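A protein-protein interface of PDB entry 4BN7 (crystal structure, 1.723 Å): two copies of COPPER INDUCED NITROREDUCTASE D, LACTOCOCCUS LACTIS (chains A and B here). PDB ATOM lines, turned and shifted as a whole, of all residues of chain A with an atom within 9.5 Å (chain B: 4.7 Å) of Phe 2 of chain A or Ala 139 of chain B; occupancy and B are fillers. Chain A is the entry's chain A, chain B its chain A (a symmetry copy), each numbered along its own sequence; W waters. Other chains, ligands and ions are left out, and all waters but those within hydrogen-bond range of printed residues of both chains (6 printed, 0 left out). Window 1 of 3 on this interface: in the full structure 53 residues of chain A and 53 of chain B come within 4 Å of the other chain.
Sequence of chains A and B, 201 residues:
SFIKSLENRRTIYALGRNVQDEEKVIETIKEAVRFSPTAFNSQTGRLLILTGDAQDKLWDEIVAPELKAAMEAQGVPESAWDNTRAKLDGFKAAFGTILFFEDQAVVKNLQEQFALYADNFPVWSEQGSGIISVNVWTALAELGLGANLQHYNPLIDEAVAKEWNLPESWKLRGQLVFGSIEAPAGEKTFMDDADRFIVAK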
ATOM      1  N   SER A   1      22.948  11.403  25.158  1.00  0.00           N
ATOM      2  CA  SER A   1      23.779  10.924  24.063  1.00  0.00           C
ATOM      3  C   SER A   1      23.539  11.748  22.799  1.00  0.00           C
ATOM      4  O   SER A   1      22.563  12.506  22.691  1.00  0.00           O
ATOM      5  CB  SER A   1      23.510   9.433  23.775  1.00  0.00           C
ATOM      6  OG  SER A   1      22.311   9.231  23.006  1.00  0.00           O
ATOM      7  N   PHE A   2      24.447  11.605  21.844  1.00  0.00           N
ATOM      8  CA  PHE A   2      24.320  12.278  20.562  1.00  0.00           C
ATOM      9  C   PHE A   2      23.105  11.765  19.787  1.00  0.00           C
ATOM     10  O   PHE A   2      22.350  12.552  19.201  1.00  0.00           O
ATOM     11  CB  PHE A   2      25.591  12.075  19.729  1.00  0.00           C
ATOM     12  CG  PHE A   2      25.525  12.707  18.377  1.00  0.00           C
ATOM     13  CD1 PHE A   2      25.570  14.086  18.244  1.00  0.00           C
ATOM     14  CD2 PHE A   2      25.383  11.938  17.241  1.00  0.00           C
ATOM     15  CE1 PHE A   2      25.484  14.673  17.002  1.00  0.00           C
ATOM     16  CE2 PHE A   2      25.296  12.525  15.992  1.00  0.00           C
ATOM     17  CZ  PHE A   2      25.347  13.901  15.878  1.00  0.00           C
ATOM     18  N   ILE A   3      22.909  10.448  19.776  1.00  0.00           N
ATOM     19  CA  ILE A   3      21.747   9.905  19.077  1.00  0.00           C
ATOM     20  C   ILE A   3      20.454  10.429  19.708  1.00  0.00           C
ATOM     21  O   ILE A   3      19.534  10.793  18.993  1.00  0.00           O
ATOM     22  CB  ILE A   3      21.759   8.373  19.027  1.00  0.00           C
ATOM     23  CG1 ILE A   3      22.946   7.873  18.184  1.00  0.00           C
ATOM     24  CG2 ILE A   3      20.452   7.852  18.468  1.00  0.00           C
ATOM     25  CD1 ILE A   3      22.869   8.246  16.698  1.00  0.00           C
ATOM     26  N   LYS A   4      20.393  10.488  21.036  1.00  0.00           N
ATOM     27  CA  LYS A   4      19.225  11.063  21.704  1.00  0.00           C
ATOM     28  C   LYS A   4      18.996  12.517  21.284  1.00  0.00           C
ATOM     29  O   LYS A   4      17.853  12.944  21.109  1.00  0.00           O
ATOM     30  CB  LYS A   4      19.353  10.971  23.233  1.00  0.00           C
ATOM     31  CG  LYS A   4      19.424   9.558  23.798  1.00  0.00           C
ATOM     32  CD  LYS A   4      18.570   8.568  23.021  1.00  0.00           C
ATOM     33  CE  LYS A   4      18.832   7.140  23.479  1.00  0.00           C
ATOM     34  NZ  LYS A   4      18.039   6.149  22.701  1.00  0.00           N
ATOM     35  N   SER A   5      20.073  13.285  21.120  1.00  0.00           N
ATOM     36  CA  SER A   5      19.943  14.665  20.674  1.00  0.00           C
ATOM     37  C   SER A   5      19.333  14.720  19.279  1.00  0.00           C
ATOM     38  O   SER A   5      18.479  15.566  19.005  1.00  0.00           O
ATOM     39  CB  SER A   5      21.296  15.392  20.682  1.00  0.00           C
ATOM     40  OG  SER A   5      21.832  15.469  21.996  1.00  0.00           O
ATOM     41  N   LEU A   6      19.767  13.823  18.396  1.00  0.00           N
ATOM     42  CA  LEU A   6      19.210  13.772  17.044  1.00  0.00           C
ATOM     43  C   LEU A   6      17.725  13.434  17.062  1.00  0.00           C
ATOM     44  O   LEU A   6      16.930  14.042  16.347  1.00  0.00           O
ATOM     45  CB  LEU A   6      19.950  12.747  16.183  1.00  0.00           C
ATOM     46  CG  LEU A   6      21.419  13.025  15.856  1.00  0.00           C
ATOM     47  CD1 LEU A   6      21.936  11.933  14.948  1.00  0.00           C
ATOM     48  CD2 LEU A   6      21.604  14.403  15.207  1.00  0.00           C
ATOM     49  N   GLU A   7      17.358  12.455  17.879  1.00  0.00           N
ATOM     50  CA  GLU A   7      15.979  12.020  17.958  1.00  0.00           C
ATOM     51  C   GLU A   7      15.095  13.137  18.521  1.00  0.00           C
ATOM     52  O   GLU A   7      13.932  13.263  18.144  1.00  0.00           O
ATOM     53  CB  GLU A   7      15.874  10.749  18.811  1.00  0.00           C
ATOM     54  CG  GLU A   7      14.561  10.016  18.653  1.00  0.00           C
ATOM     55  CD  GLU A   7      14.484   8.759  19.493  1.00  0.00           C
ATOM     56  OE1 GLU A   7      15.483   8.418  20.165  1.00  0.00           O
ATOM     57  OE2 GLU A   7      13.415   8.117  19.481  1.00  0.00           O
ATOM     58  N   ASN A   8      15.662  13.956  19.401  1.00  0.00           N
ATOM     59  CA  ASN A   8      14.911  15.042  20.021  1.00  0.00           C
ATOM     60  C   ASN A   8      14.585  16.200  19.076  1.00  0.00           C
ATOM     61  O   ASN A   8      13.629  16.938  19.309  1.00  0.00           O
ATOM     62  CB  ASN A   8      15.651  15.573  21.245  1.00  0.00           C
ATOM     63  CG  ASN A   8      14.811  16.537  22.056  1.00  0.00           C
ATOM     64  OD1 ASN A   8      13.722  16.186  22.521  1.00  0.00           O
ATOM     65  ND2 ASN A   8      15.309  17.750  22.239  1.00  0.00           N
ATOM     66  N   ARG A   9      15.364  16.362  18.013  1.00  0.00           N
ATOM     67  CA  ARG A   9      15.093  17.418  17.043  1.00  0.00           C
ATOM     68  C   ARG A   9      13.889  17.008  16.206  1.00  0.00           C
ATOM     69  O   ARG A   9      13.866  15.924  15.630  1.00  0.00           O
ATOM     70  CB  ARG A   9      16.305  17.671  16.139  1.00  0.00           C
ATOM     71  CG  ARG A   9      16.101  18.759  15.079  1.00  0.00           C
ATOM     72  CD  ARG A   9      16.694  18.374  13.737  1.00  0.00           C
ATOM     73  NE  ARG A   9      16.192  17.071  13.315  1.00  0.00           N
ATOM     74  CZ  ARG A   9      15.003  16.856  12.756  1.00  0.00           C
ATOM     75  NH1 ARG A   9      14.172  17.861  12.501  1.00  0.00           N
ATOM     76  NH2 ARG A   9      14.643  15.621  12.442  1.00  0.00           N
ATOM     77  N   VAL A 134      20.780  21.737   9.913  1.00  0.00           N
ATOM     78  CA  VAL A 134      20.342  20.725  10.871  1.00  0.00           C
ATOM     79  C   VAL A 134      21.142  20.766  12.166  1.00  0.00           C
ATOM     80  O   VAL A 134      20.595  20.473  13.232  1.00  0.00           O
ATOM     81  CB  VAL A 134      20.332  19.293  10.294  1.00  0.00           C
ATOM     82  CG1 VAL A 134      19.463  19.242   9.047  1.00  0.00           C
ATOM     83  CG2 VAL A 134      21.748  18.797  10.024  1.00  0.00           C
ATOM     84  N   ASN A 135      22.420  21.137  12.098  1.00  0.00           N
ATOM     85  CA  ASN A 135      23.182  21.306  13.329  1.00  0.00           C
ATOM     86  C   ASN A 135      22.617  22.426  14.213  1.00  0.00           C
ATOM     87  O   ASN A 135      22.495  22.256  15.426  1.00  0.00           O
ATOM     88  CB  ASN A 135      24.672  21.502  13.041  1.00  0.00           C
ATOM     89  CG  ASN A 135      25.385  20.187  12.802  1.00  0.00           C
ATOM     90  OD1 ASN A 135      24.845  19.120  13.111  1.00  0.00           O
ATOM     91  ND2 ASN A 135      26.599  20.246  12.258  1.00  0.00           N
ATOM     92  N   THR A 138      19.192  21.188  15.585  1.00  0.00           N
ATOM     93  CA  THR A 138      19.353  20.241  16.676  1.00  0.00           C
ATOM     94  C   THR A 138      19.863  20.937  17.937  1.00  0.00           C
ATOM     95  O   THR A 138      19.435  20.614  19.036  1.00  0.00           O
ATOM     96  CB  THR A 138      20.289  19.076  16.279  1.00  0.00           C
ATOM     97  OG1 THR A 138      19.787  18.432  15.095  1.00  0.00           O
ATOM     98  CG2 THR A 138      20.381  18.046  17.397  1.00  0.00           C
ATOM     99  N   ALA A 139      20.765  21.903  17.777  1.00  0.00           N
ATOM    100  CA  ALA A 139      21.268  22.648  18.925  1.00  0.00           C
ATOM    101  C   ALA A 139      20.138  23.423  19.619  1.00  0.00           C
ATOM    102  O   ALA A 139      20.058  23.477  20.846  1.00  0.00           O
ATOM    103  CB  ALA A 139      22.378  23.577  18.496  1.00  0.00           C
ATOM    104  N   GLU A 142      18.070  21.152  21.704  1.00  0.00           N
ATOM    105  CA  GLU A 142      18.715  20.809  22.963  1.00  0.00           C
ATOM    106  C   GLU A 142      18.487  21.902  24.016  1.00  0.00           C
ATOM    107  O   GLU A 142      18.502  21.626  25.220  1.00  0.00           O
ATOM    108  CB  GLU A 142      20.201  20.520  22.751  1.00  0.00           C
ATOM    109  CG  GLU A 142      20.468  19.177  22.063  1.00  0.00           C
ATOM    110  CD  GLU A 142      20.102  17.973  22.934  1.00  0.00           C
ATOM    111  OE1 GLU A 142      18.938  17.508  22.874  1.00  0.00           O
ATOM    112  OE2 GLU A 142      20.985  17.489  23.679  1.00  0.00           O
ATOM    113  N   PHE B   2      25.538  18.646  23.156  1.00  0.00           N
ATOM    114  CA  PHE B   2      25.470  18.512  21.711  1.00  0.00           C
ATOM    115  C   PHE B   2      26.581  19.312  21.028  1.00  0.00           C
ATOM    116  O   PHE B   2      27.227  18.826  20.091  1.00  0.00           O
ATOM    117  CB  PHE B   2      24.103  18.980  21.198  1.00  0.00           C
ATOM    118  CG  PHE B   2      23.967  18.908  19.712  1.00  0.00           C
ATOM    119  CD1 PHE B   2      23.867  17.681  19.075  1.00  0.00           C
ATOM    120  CD2 PHE B   2      23.973  20.053  18.943  1.00  0.00           C
ATOM    121  CE1 PHE B   2      23.767  17.609  17.704  1.00  0.00           C
ATOM    122  CE2 PHE B   2      23.873  19.985  17.566  1.00  0.00           C
ATOM    123  CZ  PHE B   2      23.769  18.752  16.949  1.00  0.00           C
ATOM    124  N   SER B   5      29.725  17.483  21.261  1.00  0.00           N
ATOM    125  CA  SER B   5      29.755  16.379  20.313  1.00  0.00           C
ATOM    126  C   SER B   5      30.167  16.871  18.931  1.00  0.00           C
ATOM    127  O   SER B   5      30.953  16.215  18.244  1.00  0.00           O
ATOM    128  CB  SER B   5      28.397  15.666  20.230  1.00  0.00           C
ATOM    129  OG  SER B   5      28.044  15.084  21.477  1.00  0.00           O
ATOM    130  N   LEU B   6      29.641  18.023  18.521  1.00  0.00           N
ATOM    131  CA  LEU B   6      30.010  18.597  17.226  1.00  0.00           C
ATOM    132  C   LEU B   6      31.491  18.942  17.168  1.00  0.00           C
ATOM    133  O   LEU B   6      32.164  18.672  16.175  1.00  0.00           O
ATOM    134  CB  LEU B   6      29.187  19.851  16.926  1.00  0.00           C
ATOM    135  CG  LEU B   6      27.680  19.678  16.723  1.00  0.00           C
ATOM    136  CD1 LEU B   6      27.073  21.017  16.375  1.00  0.00           C
ATOM    137  CD2 LEU B   6      27.371  18.643  15.633  1.00  0.00           C
ATOM    138  N   THR B  28      24.773   2.269  15.445  1.00  0.00           N
ATOM    139  CA  THR B  28      24.872   3.711  15.588  1.00  0.00           C
ATOM    140  C   THR B  28      24.789   4.425  14.240  1.00  0.00           C
ATOM    141  O   THR B  28      24.165   5.481  14.122  1.00  0.00           O
ATOM    142  CB  THR B  28      26.167   4.081  16.323  1.00  0.00           C
ATOM    143  OG1 THR B  28      26.223   3.363  17.562  1.00  0.00           O
ATOM    144  CG2 THR B  28      26.211   5.553  16.613  1.00  0.00           C
ATOM    145  N   ALA B  32      21.876   7.152  13.310  1.00  0.00           N
ATOM    146  CA  ALA B  32      22.192   8.514  12.894  1.00  0.00           C
ATOM    147  C   ALA B  32      21.443   8.899  11.617  1.00  0.00           C
ATOM    148  O   ALA B  32      20.940  10.021  11.495  1.00  0.00           O
ATOM    149  CB  ALA B  32      23.706   8.697  12.713  1.00  0.00           C
ATOM    150  N   ASN B 135      25.957  13.565  10.351  1.00  0.00           N
ATOM    151  CA  ASN B 135      25.366  12.923  11.518  1.00  0.00           C
ATOM    152  C   ASN B 135      26.016  11.568  11.828  1.00  0.00           C
ATOM    153  O   ASN B 135      26.307  11.269  12.985  1.00  0.00           O
ATOM    154  CB  ASN B 135      23.846  12.810  11.385  1.00  0.00           C
ATOM    155  CG  ASN B 135      23.142  14.098  11.761  1.00  0.00           C
ATOM    156  OD1 ASN B 135      23.748  14.983  12.372  1.00  0.00           O
ATOM    157  ND2 ASN B 135      21.865  14.217  11.405  1.00  0.00           N
ATOM    158  N   VAL B 136      26.262  10.758  10.806  1.00  0.00           N
ATOM    159  CA  VAL B 136      26.988   9.503  10.993  1.00  0.00           C
ATOM    160  C   VAL B 136      28.429   9.768  11.476  1.00  0.00           C
ATOM    161  O   VAL B 136      28.908   9.140  12.428  1.00  0.00           O
ATOM    162  CB  VAL B 136      27.014   8.680   9.699  1.00  0.00           C
ATOM    163  CG1 VAL B 136      27.988   7.518   9.832  1.00  0.00           C
ATOM    164  CG2 VAL B 136      25.625   8.172   9.357  1.00  0.00           C
ATOM    165  N   TRP B 137      29.096  10.711  10.820  1.00  0.00           N
ATOM    166  CA  TRP B 137      30.472  11.092  11.146  1.00  0.00           C
ATOM    167  C   TRP B 137      30.561  11.458  12.628  1.00  0.00           C
ATOM    168  O   TRP B 137      31.446  10.992  13.349  1.00  0.00           O
ATOM    169  CB  TRP B 137      30.853  12.286  10.278  1.00  0.00           C
ATOM    170  CG  TRP B 137      32.307  12.626  10.135  1.00  0.00           C
ATOM    171  CD1 TRP B 137      33.363  12.172  10.881  1.00  0.00           C
ATOM    172  CD2 TRP B 137      32.855  13.508   9.159  1.00  0.00           C
ATOM    173  NE1 TRP B 137      34.538  12.729  10.419  1.00  0.00           N
ATOM    174  CE2 TRP B 137      34.249  13.545   9.355  1.00  0.00           C
ATOM    175  CE3 TRP B 137      32.296  14.266   8.127  1.00  0.00           C
ATOM    176  CZ2 TRP B 137      35.086  14.328   8.569  1.00  0.00           C
ATOM    177  CZ3 TRP B 137      33.122  15.033   7.351  1.00  0.00           C
ATOM    178  CH2 TRP B 137      34.509  15.058   7.567  1.00  0.00           C
ATOM    179  N   THR B 138      29.628  12.286  13.084  1.00  0.00           N
ATOM    180  CA  THR B 138      29.644  12.746  14.463  1.00  0.00           C
ATOM    181  C   THR B 138      29.292  11.611  15.424  1.00  0.00           C
ATOM    182  O   THR B 138      29.874  11.507  16.494  1.00  0.00           O
ATOM    183  CB  THR B 138      28.694  13.949  14.667  1.00  0.00           C
ATOM    184  OG1 THR B 138      29.046  15.006  13.759  1.00  0.00           O
ATOM    185  CG2 THR B 138      28.783  14.477  16.094  1.00  0.00           C
ATOM    186  N   ALA B 139      28.351  10.753  15.036  1.00  0.00           N
ATOM    187  CA  ALA B 139      27.989   9.617  15.873  1.00  0.00           C
ATOM    188  C   ALA B 139      29.182   8.667  16.062  1.00  0.00           C
ATOM    189  O   ALA B 139      29.428   8.155  17.154  1.00  0.00           O
ATOM    190  CB  ALA B 139      26.806   8.889  15.282  1.00  0.00           C
ATOM    191  N   LEU B 140      29.924   8.440  14.993  1.00  0.00           N
ATOM    192  CA  LEU B 140      31.139   7.619  15.077  1.00  0.00           C
ATOM    193  C   LEU B 140      32.170   8.235  16.029  1.00  0.00           C
ATOM    194  O   LEU B 140      32.802   7.532  16.823  1.00  0.00           O
ATOM    195  CB  LEU B 140      31.740   7.423  13.682  1.00  0.00           C
ATOM    196  CG  LEU B 140      30.915   6.552  12.717  1.00  0.00           C
ATOM    197  CD1 LEU B 140      31.494   6.625  11.322  1.00  0.00           C
ATOM    198  CD2 LEU B 140      30.853   5.108  13.181  1.00  0.00           C
ATOM    199  N   ALA B 141      32.352   9.550  15.944  1.00  0.00           N
ATOM    200  CA  ALA B 141      33.290  10.233  16.818  1.00  0.00           C
ATOM    201  C   ALA B 141      32.880  10.069  18.279  1.00  0.00           C
ATOM    202  O   ALA B 141      33.731   9.970  19.157  1.00  0.00           O
ATOM    203  CB  ALA B 141      33.396  11.713  16.448  1.00  0.00           C
ATOM    204  N   GLU B 142      31.576  10.036  18.547  1.00  0.00           N
ATOM    205  CA  GLU B 142      31.119   9.860  19.917  1.00  0.00           C
ATOM    206  C   GLU B 142      31.458   8.457  20.437  1.00  0.00           C
ATOM    207  O   GLU B 142      31.616   8.256  21.646  1.00  0.00           O
ATOM    208  CB  GLU B 142      29.626  10.168  20.035  1.00  0.00           C
ATOM    209  CG  GLU B 142      29.304  11.663  19.950  1.00  0.00           C
ATOM    210  CD  GLU B 142      29.817  12.458  21.153  1.00  0.00           C
ATOM    211  OE1 GLU B 142      30.974  12.943  21.114  1.00  0.00           O
ATOM    212  OE2 GLU B 142      29.057  12.600  22.139  1.00  0.00           O
ATOM    213  N   LEU B 143      31.608   7.495  19.528  1.00  0.00           N
ATOM    214  CA  LEU B 143      32.079   6.159  19.900  1.00  0.00           C
ATOM    215  C   LEU B 143      33.595   6.100  20.059  1.00  0.00           C
ATOM    216  O   LEU B 143      34.142   5.059  20.424  1.00  0.00           O
ATOM    217  CB  LEU B 143      31.663   5.120  18.859  1.00  0.00           C
ATOM    218  CG  LEU B 143      30.168   4.845  18.692  1.00  0.00           C
ATOM    219  CD1 LEU B 143      29.954   3.772  17.639  1.00  0.00           C
ATOM    220  CD2 LEU B 143      29.553   4.435  20.009  1.00  0.00           C
HETATM  221  O   HOH W   1      20.150  16.368  12.473  1.00  0.00           O
HETATM  222  O   HOH W   2      23.025  19.331  24.546  1.00  0.00           O
HETATM  223  O   HOH W   3      27.106  10.514  22.515  1.00  0.00           O
HETATM  224  O   HOH W   4      22.622  17.406  13.471  1.00  0.00           O
HETATM  225  O   HOH W   5      26.045  16.493  13.047  1.00  0.00           O
HETATM  226  O   HOH W   6      28.384  17.898  12.188  1.00  0.00           O
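The backbone carbonyl oxygen of Ser 1 of chain A is in hydrogen-bond range of the side-chain hydroxyl of Ser 5 of chain A (3.1 Å). OG of Ser 5 of chain A lies within hydrogen-bond range of OE2 of Glu 142 of chain A, 2.8 Å away. The side-chain hydroxyl of Thr 138 of chain A is in hydrogen-bond range of the backbone carbonyl oxygen of Val 134 of chain A (2.9 Å). OG of Ser 5 of chain B is in hydrogen-bond range of OE2 of Glu 142 of chain B (2.8 Å).
Among the printed residues, pairs that only touch across the chains: Asn 135 of chain A with Phe 2 of chain B, Phe 2 of chain A with Asn 135 of chain B, Phe 2 of chain A with Thr 138 of chain B, Thr 138 of chain A with Phe 2 of chain B, Phe 2 of chain A with Phe 2 of chain B, Asn 135 of chain A with Leu 6 of chain B, Leu 6 of chain A with Asn 135 of chain B, Ala 139 of chain A with Phe 2 of chain B, Phe 2 of chain A with Ala 139 of chain B, Ile 3 of chain A with Ala 32 of chain B, Glu 142 of chain A with Phe 2 of chain B, Phe 2 of chain A with Glu 142 of chain B, Ser 5 of chain A with Phe 2 of chain B, Phe 2 of chain A with Ser 5 of chain B, Ile 3 of chain A with Thr 28 of chain B and Leu 6 of chain A with Ala 32 of chain B.
Phe 2 of chain A touches just these residues of chain B: Phe 2, Ser 5, Asn 135, Thr 138, Ala 139 and Glu 142. Of the printed residues of chain B, Leu 6 of chain A touches Ala 32 (3.997 Å) and Asn 135 (3.6 Å). Asn 8 of chain A touches none of the printed residues of chain B. Of the printed residues of chain B, Thr 138 of chain A touches Phe 2. Thr 138 of chain B touches one residue of chain A. Of chain A, only Phe 2 (3.7 Å) comes within 4 Å of Ala 139 of chain B. No residue of chain A comes within 4 Å of Ala 141 of chain B. Leu 143 of chain B touches none of the printed residues of chain A. The nearest residue of chain B that does not touch Phe 2 of chain A is Leu 6 of chain B (4.6 Å). The nearest printed residue of chain A that does not touch Asn 135 of chain B is Asn 135 of chain A (4.3 Å).
Of the 14 printed residues of chain A, 8 touch a printed residue of chain B. Hydrophobic or aromatic side chains of chain B that line the printed part of chain A: Phe 2, Leu 6 and Ala 139. Along chain B the printed residues that touch a printed residue of chain A span positions 2 to 142. Among the printed residues, 16 pairs touch across the chains.
Phe 2 of chain B touches its own counterpart, Phe 2 of chain A. Phe 2 of chain A touches Asn 135 of chain B, and with the chains exchanged Asn 135 of chain A touches Phe 2 of chain B. Phe 2 of chain A touches Ala 139 of chain B, and with the chains exchanged Ala 139 of chain A touches Phe 2 of chain B. Phe 2 of chain A touches Glu 142 of chain B, and with the chains exchanged Glu 142 of chain A touches Phe 2 of chain B. Positions printed for both chains: 2, 5, 6, 135, 138, 139 and 142. Of the 16 pairs that touch across the chains among the printed residues, 13 have their exchanged pair printed and touching as well.
Water W5 lies within hydrogen-bond range of the side-chain amide oxygen of Asn 135 of chain B (2.8 Å), the side-chain amide oxygen of Asn 135 of chain A (2.9 Å) and the side-chain hydroxyl of Thr 138 of chain B (3.4 Å). Water W4 lies within hydrogen-bond range of OD1 of Asn 135 of chain A (2.8 Å), OD1 of Asn 135 of chain B (2.9 Å) and OG1 of Thr 138 of chain A (3.4 Å). Water W2 bridges OE2 of Glu 142 of chain A (2.9 Å) and N of Phe 2 of chain B (3.0 Å). Water W3 lies within hydrogen-bond range of the side-chain carboxylate (OE2) of Glu 142 of chain B and the backbone NH (N) of Phe 2 of chain A. Water W1 bridges the side-chain amide nitrogen of Asn 135 of chain B and the side-chain hydroxyl of Thr 138 of chain A. Water W6 lies within hydrogen-bond range of the side-chain amide nitrogen (ND2) of Asn 135 of chain A (3.0 Å) and the side-chain hydroxyl (OG1) of Thr 138 of chain B (3.4 Å).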
